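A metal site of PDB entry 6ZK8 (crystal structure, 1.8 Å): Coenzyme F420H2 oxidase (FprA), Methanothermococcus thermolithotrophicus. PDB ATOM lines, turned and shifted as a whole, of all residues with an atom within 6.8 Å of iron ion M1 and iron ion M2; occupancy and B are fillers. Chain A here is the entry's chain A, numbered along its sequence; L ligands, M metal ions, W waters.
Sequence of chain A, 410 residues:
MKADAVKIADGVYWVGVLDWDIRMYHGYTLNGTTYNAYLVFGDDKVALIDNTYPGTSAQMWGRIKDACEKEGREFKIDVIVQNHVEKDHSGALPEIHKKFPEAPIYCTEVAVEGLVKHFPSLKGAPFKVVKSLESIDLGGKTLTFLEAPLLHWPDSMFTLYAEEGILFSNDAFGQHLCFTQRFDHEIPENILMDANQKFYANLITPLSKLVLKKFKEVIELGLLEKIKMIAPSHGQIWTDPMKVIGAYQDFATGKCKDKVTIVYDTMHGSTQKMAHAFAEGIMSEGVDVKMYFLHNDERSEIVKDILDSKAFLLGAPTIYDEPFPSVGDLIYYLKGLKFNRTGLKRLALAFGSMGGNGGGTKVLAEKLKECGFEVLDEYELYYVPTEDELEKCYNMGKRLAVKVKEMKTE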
ATOM      1  N   TYR A  25     -27.999 -30.352   8.903  1.00  0.00           N
ATOM      2  CA  TYR A  25     -28.704 -29.073   8.843  1.00  0.00           C
ATOM      3  C   TYR A  25     -29.531 -29.103   7.565  1.00  0.00           C
ATOM      4  O   TYR A  25     -29.101 -29.680   6.560  1.00  0.00           O
ATOM      5  CB  TYR A  25     -27.721 -27.901   8.828  1.00  0.00           C
ATOM      6  CG  TYR A  25     -28.327 -26.557   9.176  1.00  0.00           C
ATOM      7  CD1 TYR A  25     -28.895 -26.342  10.407  1.00  0.00           C
ATOM      8  CD2 TYR A  25     -28.322 -25.497   8.269  1.00  0.00           C
ATOM      9  CE1 TYR A  25     -29.451 -25.118  10.741  1.00  0.00           C
ATOM     10  CE2 TYR A  25     -28.861 -24.252   8.613  1.00  0.00           C
ATOM     11  CZ  TYR A  25     -29.423 -24.082   9.867  1.00  0.00           C
ATOM     12  OH  TYR A  25     -29.988 -22.876  10.236  1.00  0.00           O
ATOM     13  N   HIS A  26     -30.699 -28.448   7.588  1.00  0.00           N
ATOM     14  CA  HIS A  26     -31.660 -28.452   6.460  1.00  0.00           C
ATOM     15  C   HIS A  26     -31.931 -29.924   6.179  1.00  0.00           C
ATOM     16  O   HIS A  26     -32.199 -30.680   7.129  1.00  0.00           O
ATOM     17  CB  HIS A  26     -31.097 -27.685   5.276  1.00  0.00           C
ATOM     18  CG  HIS A  26     -30.832 -26.233   5.525  1.00  0.00           C
ATOM     19  ND1 HIS A  26     -29.828 -25.548   4.858  1.00  0.00           N
ATOM     20  CD2 HIS A  26     -31.445 -25.324   6.317  1.00  0.00           C
ATOM     21  CE1 HIS A  26     -29.856 -24.277   5.225  1.00  0.00           C
ATOM     22  NE2 HIS A  26     -30.813 -24.118   6.126  1.00  0.00           N
ATOM     23  N   TYR A  28     -29.387 -31.916   4.892  1.00  0.00           N
ATOM     24  CA  TYR A  28     -28.095 -32.357   4.414  1.00  0.00           C
ATOM     25  C   TYR A  28     -27.129 -32.583   5.552  1.00  0.00           C
ATOM     26  O   TYR A  28     -27.339 -32.232   6.708  1.00  0.00           O
ATOM     27  CB  TYR A  28     -27.475 -31.416   3.358  1.00  0.00           C
ATOM     28  CG  TYR A  28     -27.410 -29.971   3.752  1.00  0.00           C
ATOM     29  CD1 TYR A  28     -26.578 -29.550   4.743  1.00  0.00           C
ATOM     30  CD2 TYR A  28     -28.193 -29.019   3.111  1.00  0.00           C
ATOM     31  CE1 TYR A  28     -26.555 -28.216   5.117  1.00  0.00           C
ATOM     32  CE2 TYR A  28     -28.139 -27.676   3.456  1.00  0.00           C
ATOM     33  CZ  TYR A  28     -27.321 -27.297   4.459  1.00  0.00           C
ATOM     34  OH  TYR A  28     -27.267 -25.967   4.831  1.00  0.00           O
ATOM     35  N   TYR A  35     -20.534 -19.939  10.590  1.00  0.00           N
ATOM     36  CA  TYR A  35     -21.515 -18.863  10.425  1.00  0.00           C
ATOM     37  C   TYR A  35     -20.642 -17.609  10.319  1.00  0.00           C
ATOM     38  O   TYR A  35     -20.170 -17.099  11.338  1.00  0.00           O
ATOM     39  CB  TYR A  35     -22.531 -18.806  11.578  1.00  0.00           C
ATOM     40  CG  TYR A  35     -23.089 -20.189  11.859  1.00  0.00           C
ATOM     41  CD1 TYR A  35     -23.789 -20.880  10.890  1.00  0.00           C
ATOM     42  CD2 TYR A  35     -22.862 -20.833  13.064  1.00  0.00           C
ATOM     43  CE1 TYR A  35     -24.226 -22.177  11.110  1.00  0.00           C
ATOM     44  CE2 TYR A  35     -23.327 -22.089  13.306  1.00  0.00           C
ATOM     45  CZ  TYR A  35     -23.999 -22.762  12.334  1.00  0.00           C
ATOM     46  OH  TYR A  35     -24.431 -24.018  12.541  1.00  0.00           O
ATOM     47  N   HIS A  84     -30.231 -11.634   5.603  1.00  0.00           N
ATOM     48  CA  HIS A  84     -30.982 -12.871   5.469  1.00  0.00           C
ATOM     49  C   HIS A  84     -31.547 -13.175   6.836  1.00  0.00           C
ATOM     50  O   HIS A  84     -30.848 -13.010   7.838  1.00  0.00           O
ATOM     51  CB  HIS A  84     -30.050 -13.971   4.932  1.00  0.00           C
ATOM     52  CG  HIS A  84     -30.681 -15.316   4.766  1.00  0.00           C
ATOM     53  ND1 HIS A  84     -32.005 -15.478   4.415  1.00  0.00           N
ATOM     54  CD2 HIS A  84     -30.165 -16.566   4.855  1.00  0.00           C
ATOM     55  CE1 HIS A  84     -32.283 -16.772   4.322  1.00  0.00           C
ATOM     56  NE2 HIS A  84     -31.176 -17.451   4.577  1.00  0.00           N
ATOM     57  N   GLU A  86     -32.918 -16.148   7.994  1.00  0.00           N
ATOM     58  CA  GLU A  86     -32.767 -17.499   8.542  1.00  0.00           C
ATOM     59  C   GLU A  86     -31.831 -17.493   9.750  1.00  0.00           C
ATOM     60  O   GLU A  86     -30.826 -16.792   9.760  1.00  0.00           O
ATOM     61  CB  GLU A  86     -32.251 -18.462   7.458  1.00  0.00           C
ATOM     62  CG  GLU A  86     -32.314 -19.893   7.883  1.00  0.00           C
ATOM     63  CD  GLU A  86     -32.242 -20.922   6.765  1.00  0.00           C
ATOM     64  OE1 GLU A  86     -32.445 -22.127   7.070  1.00  0.00           O
ATOM     65  OE2 GLU A  86     -32.024 -20.542   5.598  1.00  0.00           O
ATOM     66  N   LYS A  87     -32.155 -18.298  10.755  1.00  0.00           N
ATOM     67  CA  LYS A  87     -31.607 -18.057  12.075  1.00  0.00           C
ATOM     68  C   LYS A  87     -30.141 -18.465  12.211  1.00  0.00           C
ATOM     69  O   LYS A  87     -29.524 -18.104  13.221  1.00  0.00           O
ATOM     70  CB  LYS A  87     -32.467 -18.760  13.130  1.00  0.00           C
ATOM     71  CG  LYS A  87     -32.517 -20.244  13.117  1.00  0.00           C
ATOM     72  CD  LYS A  87     -33.738 -20.706  13.964  1.00  0.00           C
ATOM     73  CE  LYS A  87     -33.402 -21.775  14.948  1.00  0.00           C
ATOM     74  NZ  LYS A  87     -34.525 -21.944  15.948  1.00  0.00           N
ATOM     75  N   ASP A  88     -29.552 -19.166  11.242  1.00  0.00           N
ATOM     76  CA  ASP A  88     -28.106 -19.373  11.354  1.00  0.00           C
ATOM     77  C   ASP A  88     -27.323 -18.113  11.019  1.00  0.00           C
ATOM     78  O   ASP A  88     -26.102 -18.070  11.181  1.00  0.00           O
ATOM     79  CB  ASP A  88     -27.647 -20.574  10.500  1.00  0.00           C
ATOM     80  CG  ASP A  88     -28.090 -20.473   9.055  1.00  0.00           C
ATOM     81  OD1 ASP A  88     -29.255 -20.196   8.793  1.00  0.00           O
ATOM     82  OD2 ASP A  88     -27.228 -20.683   8.177  1.00  0.00           O
ATOM     83  N   HIS A  89     -28.011 -17.062  10.580  1.00  0.00           N
ATOM     84  CA  HIS A  89     -27.368 -15.770  10.308  1.00  0.00           C
ATOM     85  C   HIS A  89     -27.987 -14.618  11.086  1.00  0.00           C
ATOM     86  O   HIS A  89     -27.419 -13.519  11.066  1.00  0.00           O
ATOM     87  CB  HIS A  89     -27.404 -15.461   8.800  1.00  0.00           C
ATOM     88  CG  HIS A  89     -26.916 -16.594   7.957  1.00  0.00           C
ATOM     89  ND1 HIS A  89     -25.611 -17.050   8.017  1.00  0.00           N
ATOM     90  CD2 HIS A  89     -27.560 -17.419   7.098  1.00  0.00           C
ATOM     91  CE1 HIS A  89     -25.482 -18.111   7.238  1.00  0.00           C
ATOM     92  NE2 HIS A  89     -26.658 -18.364   6.671  1.00  0.00           N
ATOM     93  N   HIS A 152     -31.334 -17.328  -0.995  1.00  0.00           N
ATOM     94  CA  HIS A 152     -32.310 -18.354  -1.320  1.00  0.00           C
ATOM     95  C   HIS A 152     -33.687 -18.218  -0.645  1.00  0.00           C
ATOM     96  O   HIS A 152     -34.532 -19.121  -0.757  1.00  0.00           O
ATOM     97  CB  HIS A 152     -31.743 -19.769  -0.967  1.00  0.00           C
ATOM     98  CG  HIS A 152     -31.594 -20.014   0.524  1.00  0.00           C
ATOM     99  ND1 HIS A 152     -32.080 -21.138   1.153  1.00  0.00           N
ATOM    100  CD2 HIS A 152     -30.993 -19.271   1.487  1.00  0.00           C
ATOM    101  CE1 HIS A 152     -31.808 -21.072   2.449  1.00  0.00           C
ATOM    102  NE2 HIS A 152     -31.146 -19.943   2.676  1.00  0.00           N
ATOM    103  N   TRP A 153     -33.888 -17.124   0.063  1.00  0.00           N
ATOM    104  CA  TRP A 153     -35.171 -16.784   0.658  1.00  0.00           C
ATOM    105  C   TRP A 153     -35.682 -15.458   0.094  1.00  0.00           C
ATOM    106  O   TRP A 153     -34.913 -14.669  -0.483  1.00  0.00           O
ATOM    107  CB  TRP A 153     -35.070 -16.674   2.191  1.00  0.00           C
ATOM    108  CG  TRP A 153     -35.111 -18.022   2.913  1.00  0.00           C
ATOM    109  CD1 TRP A 153     -34.927 -19.253   2.361  1.00  0.00           C
ATOM    110  CD2 TRP A 153     -35.339 -18.219   4.303  1.00  0.00           C
ATOM    111  NE1 TRP A 153     -35.021 -20.226   3.335  1.00  0.00           N
ATOM    112  CE2 TRP A 153     -35.275 -19.614   4.542  1.00  0.00           C
ATOM    113  CE3 TRP A 153     -35.594 -17.364   5.384  1.00  0.00           C
ATOM    114  CZ2 TRP A 153     -35.450 -20.171   5.810  1.00  0.00           C
ATOM    115  CZ3 TRP A 153     -35.779 -17.923   6.651  1.00  0.00           C
ATOM    116  CH2 TRP A 153     -35.703 -19.317   6.847  1.00  0.00           C
ATOM    117  N   SER A 156     -33.626 -12.314   1.088  1.00  0.00           N
ATOM    118  CA  SER A 156     -32.180 -12.306   0.949  1.00  0.00           C
ATOM    119  C   SER A 156     -31.688 -11.055   0.226  1.00  0.00           C
ATOM    120  O   SER A 156     -32.373 -10.461  -0.615  1.00  0.00           O
ATOM    121  CB  SER A 156     -31.708 -13.567   0.221  1.00  0.00           C
ATOM    122  OG  SER A 156     -32.039 -14.747   0.931  1.00  0.00           O
ATOM    123  N   ASN A 170     -24.033 -13.571   1.678  1.00  0.00           N
ATOM    124  CA  ASN A 170     -24.776 -14.456   2.598  1.00  0.00           C
ATOM    125  C   ASN A 170     -24.684 -15.883   2.064  1.00  0.00           C
ATOM    126  O   ASN A 170     -23.567 -16.304   1.755  1.00  0.00           O
ATOM    127  CB  ASN A 170     -26.189 -13.919   2.791  1.00  0.00           C
ATOM    128  CG  ASN A 170     -26.908 -14.590   3.948  1.00  0.00           C
ATOM    129  OD1 ASN A 170     -27.692 -15.534   3.759  1.00  0.00           O
ATOM    130  ND2 ASN A 170     -26.624 -14.111   5.168  1.00  0.00           N
ATOM    131  N   ASP A 171     -25.789 -16.614   1.941  1.00  0.00           N
ATOM    132  CA  ASP A 171     -25.680 -18.040   1.641  1.00  0.00           C
ATOM    133  C   ASP A 171     -25.089 -18.288   0.259  1.00  0.00           C
ATOM    134  O   ASP A 171     -24.383 -19.289   0.054  1.00  0.00           O
ATOM    135  CB  ASP A 171     -27.047 -18.732   1.733  1.00  0.00           C
ATOM    136  CG  ASP A 171     -27.518 -19.012   3.176  1.00  0.00           C
ATOM    137  OD1 ASP A 171     -26.777 -19.571   4.011  1.00  0.00           O
ATOM    138  OD2 ASP A 171     -28.673 -18.674   3.478  1.00  0.00           O
ATOM    139  N   HIS A 176     -20.325 -25.614   3.138  1.00  0.00           N
ATOM    140  CA  HIS A 176     -20.330 -26.071   4.518  1.00  0.00           C
ATOM    141  C   HIS A 176     -19.014 -26.735   4.799  1.00  0.00           C
ATOM    142  O   HIS A 176     -18.855 -27.939   4.618  1.00  0.00           O
ATOM    143  CB  HIS A 176     -21.518 -26.987   4.786  1.00  0.00           C
ATOM    144  CG  HIS A 176     -22.806 -26.255   4.905  1.00  0.00           C
ATOM    145  ND1 HIS A 176     -22.944 -25.141   5.710  1.00  0.00           N
ATOM    146  CD2 HIS A 176     -24.001 -26.439   4.306  1.00  0.00           C
ATOM    147  CE1 HIS A 176     -24.176 -24.687   5.614  1.00  0.00           C
ATOM    148  NE2 HIS A 176     -24.839 -25.461   4.759  1.00  0.00           N
ATOM    149  N   PHE A 199     -23.296 -27.718  -1.882  1.00  0.00           N
ATOM    150  CA  PHE A 199     -24.124 -26.585  -1.487  1.00  0.00           C
ATOM    151  C   PHE A 199     -25.070 -26.170  -2.611  1.00  0.00           C
ATOM    152  O   PHE A 199     -26.284 -26.068  -2.402  1.00  0.00           O
ATOM    153  CB  PHE A 199     -23.192 -25.434  -1.089  1.00  0.00           C
ATOM    154  CG  PHE A 199     -23.853 -24.348  -0.286  1.00  0.00           C
ATOM    155  CD1 PHE A 199     -24.528 -23.319  -0.903  1.00  0.00           C
ATOM    156  CD2 PHE A 199     -23.767 -24.342   1.085  1.00  0.00           C
ATOM    157  CE1 PHE A 199     -25.139 -22.330  -0.183  1.00  0.00           C
ATOM    158  CE2 PHE A 199     -24.358 -23.349   1.807  1.00  0.00           C
ATOM    159  CZ  PHE A 199     -25.032 -22.325   1.176  1.00  0.00           C
ATOM    160  N   LEU A 203     -29.133 -26.626  -2.268  1.00  0.00           N
ATOM    161  CA  LEU A 203     -29.786 -25.367  -1.926  1.00  0.00           C
ATOM    162  C   LEU A 203     -30.087 -24.458  -3.100  1.00  0.00           C
ATOM    163  O   LEU A 203     -31.037 -23.668  -3.016  1.00  0.00           O
ATOM    164  CB  LEU A 203     -28.930 -24.588  -0.917  1.00  0.00           C
ATOM    165  CG  LEU A 203     -28.802 -25.237   0.444  1.00  0.00           C
ATOM    166  CD1 LEU A 203     -27.734 -24.594   1.304  1.00  0.00           C
ATOM    167  CD2 LEU A 203     -30.148 -25.186   1.166  1.00  0.00           C
ATOM    168  N   SER A 233     -21.584 -16.479   3.787  1.00  0.00           N
ATOM    169  CA  SER A 233     -21.971 -16.696   5.182  1.00  0.00           C
ATOM    170  C   SER A 233     -21.656 -18.108   5.686  1.00  0.00           C
ATOM    171  O   SER A 233     -21.881 -18.379   6.861  1.00  0.00           O
ATOM    172  CB  SER A 233     -23.467 -16.399   5.349  1.00  0.00           C
ATOM    173  OG  SER A 233     -24.231 -17.350   4.632  1.00  0.00           O
ATOM    174  N   HIS A 234     -21.135 -18.991   4.830  1.00  0.00           N
ATOM    175  CA  HIS A 234     -20.697 -20.317   5.251  1.00  0.00           C
ATOM    176  C   HIS A 234     -19.410 -20.635   4.522  1.00  0.00           C
ATOM    177  O   HIS A 234     -19.305 -20.423   3.309  1.00  0.00           O
ATOM    178  CB  HIS A 234     -21.720 -21.427   4.919  1.00  0.00           C
ATOM    179  CG  HIS A 234     -23.049 -21.270   5.593  1.00  0.00           C
ATOM    180  ND1 HIS A 234     -23.234 -21.537   6.936  1.00  0.00           N
ATOM    181  CD2 HIS A 234     -24.250 -20.883   5.118  1.00  0.00           C
ATOM    182  CE1 HIS A 234     -24.484 -21.304   7.255  1.00  0.00           C
ATOM    183  NE2 HIS A 234     -25.135 -20.911   6.170  1.00  0.00           N
HETATM  184  N1  LIG L   1     -40.748 -21.570   2.934  1.00  0.00           N
HETATM  185  C1  LIG L   1     -41.718 -21.443   1.948  1.00  0.00           C
HETATM  186  O1  LIG L   1     -42.803 -20.958   2.232  1.00  0.00           O
HETATM  187  N2  LIG L   1     -41.458 -21.860   0.647  1.00  0.00           N
HETATM  188  C2  LIG L   1     -40.232 -22.400   0.344  1.00  0.00           C
HETATM  189  O2  LIG L   1     -39.998 -22.775  -0.802  1.00  0.00           O
HETATM  190  C3  LIG L   1     -39.253 -22.526   1.331  1.00  0.00           C
HETATM  191  N3  LIG L   1     -38.028 -23.049   1.015  1.00  0.00           N
HETATM  192  C4  LIG L   1     -37.084 -23.211   2.017  1.00  0.00           C
HETATM  193  C5  LIG L   1     -35.862 -23.788   1.719  1.00  0.00           C
HETATM  194  C6  LIG L   1     -34.899 -23.939   2.705  1.00  0.00           C
HETATM  195  C7  LIG L   1     -33.577 -24.555   2.363  1.00  0.00           C
HETATM  196  C8  LIG L   1     -35.176 -23.538   4.010  1.00  0.00           C
HETATM  197  C9  LIG L   1     -34.133 -23.712   5.071  1.00  0.00           C
HETATM  198  C10 LIG L   1     -36.408 -22.963   4.307  1.00  0.00           C
HETATM  199  C11 LIG L   1     -37.363 -22.797   3.318  1.00  0.00           C
HETATM  200  N4  LIG L   1     -38.602 -22.241   3.606  1.00  0.00           N
HETATM  201  C12 LIG L   1     -39.532 -22.103   2.613  1.00  0.00           C
HETATM  202  C13 LIG L   1     -38.948 -21.746   4.969  1.00  0.00           C
HETATM  203  C14 LIG L   1     -39.390 -22.773   5.991  1.00  0.00           C
HETATM  204  O3  LIG L   1     -40.624 -23.378   5.632  1.00  0.00           O
HETATM  205  C15 LIG L   1     -39.598 -21.968   7.281  1.00  0.00           C
HETATM  206  O4  LIG L   1     -38.339 -21.571   7.771  1.00  0.00           O
HETATM  207  C16 LIG L   1     -40.366 -22.746   8.342  1.00  0.00           C
HETATM  208  O5  LIG L   1     -40.771 -21.889   9.383  1.00  0.00           O
HETATM  209  C17 LIG L   1     -39.464 -23.844   8.909  1.00  0.00           C
HETATM  210  O6  LIG L   1     -40.233 -24.616   9.795  1.00  0.00           O
HETATM  211  P1  LIG L   1     -39.515 -25.560  10.854  1.00  0.00           P
HETATM  212  O7  LIG L   1     -38.362 -26.206  10.167  1.00  0.00           O
HETATM  213  O8  LIG L   1     -39.011 -24.709  11.973  1.00  0.00           O
HETATM  214  O9  LIG L   1     -40.536 -26.542  11.386  1.00  0.00           O
HETATM  215 FE    FE M   1     -30.221 -19.614   4.622  1.00  0.00          FE
HETATM  216 FE    FE M   2     -27.211 -20.129   5.919  1.00  0.00          FE
HETATM  217  O   HOH W   1     -29.101 -20.340   5.868  1.00  0.00           O
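A ring nitrogen (NE2) of His 89 lies close to the side-chain hydroxyl (OG) of Ser 233. OG of Ser 233 lies within hydrogen-bond range of N of Asp 171 (3.2 Å). The side-chain carboxylate (OD2) of Asp 171 sits close to the side-chain amide oxygen (OD1) of Asn 170 (3.3 Å). The backbone NH of His 152 sits at hydrogen-bond distance from the side-chain hydroxyl of Ser 156 (3.3 Å). OE1 of Glu 86 sits at hydrogen-bond distance from NE2 of His 26. The side-chain carboxylate (OD1) of Asp 88 is in hydrogen-bond range of the side-chain hydroxyl (OH) of Tyr 25 (3.1 Å).
Of the 19 residues printed, 4 come within 4 Å of iron ion M1. The nearest printed residue that does not touch iron ion M1 is His 89 (4.2 Å).
Four residues have an atom within 4 Å of iron ion M2: Asp 88, His 89, Asp 171 and His 234. The nearest printed residue that does not touch iron ion M2 is Ser 233 (4.3 Å).
Iron ion M1 is bound by water W1 (1.8 Å), the side-chain carboxylate of Asp 171 (2.1 Å), a ring nitrogen (NE2) of His 152 (2.2 Å), the side-chain carboxylate of Glu 86 (2.3 Å) and a ring nitrogen (NE2) of His 84 (2.4 Å).
Iron ion M2 is bound by water W1 (1.9 Å), NE2 of His 89 (2.0 Å), OD1 of Asp 171 (2.0 Å), NE2 of His 234 (2.2 Å) and OD2 of Asp 88 (2.3 Å).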
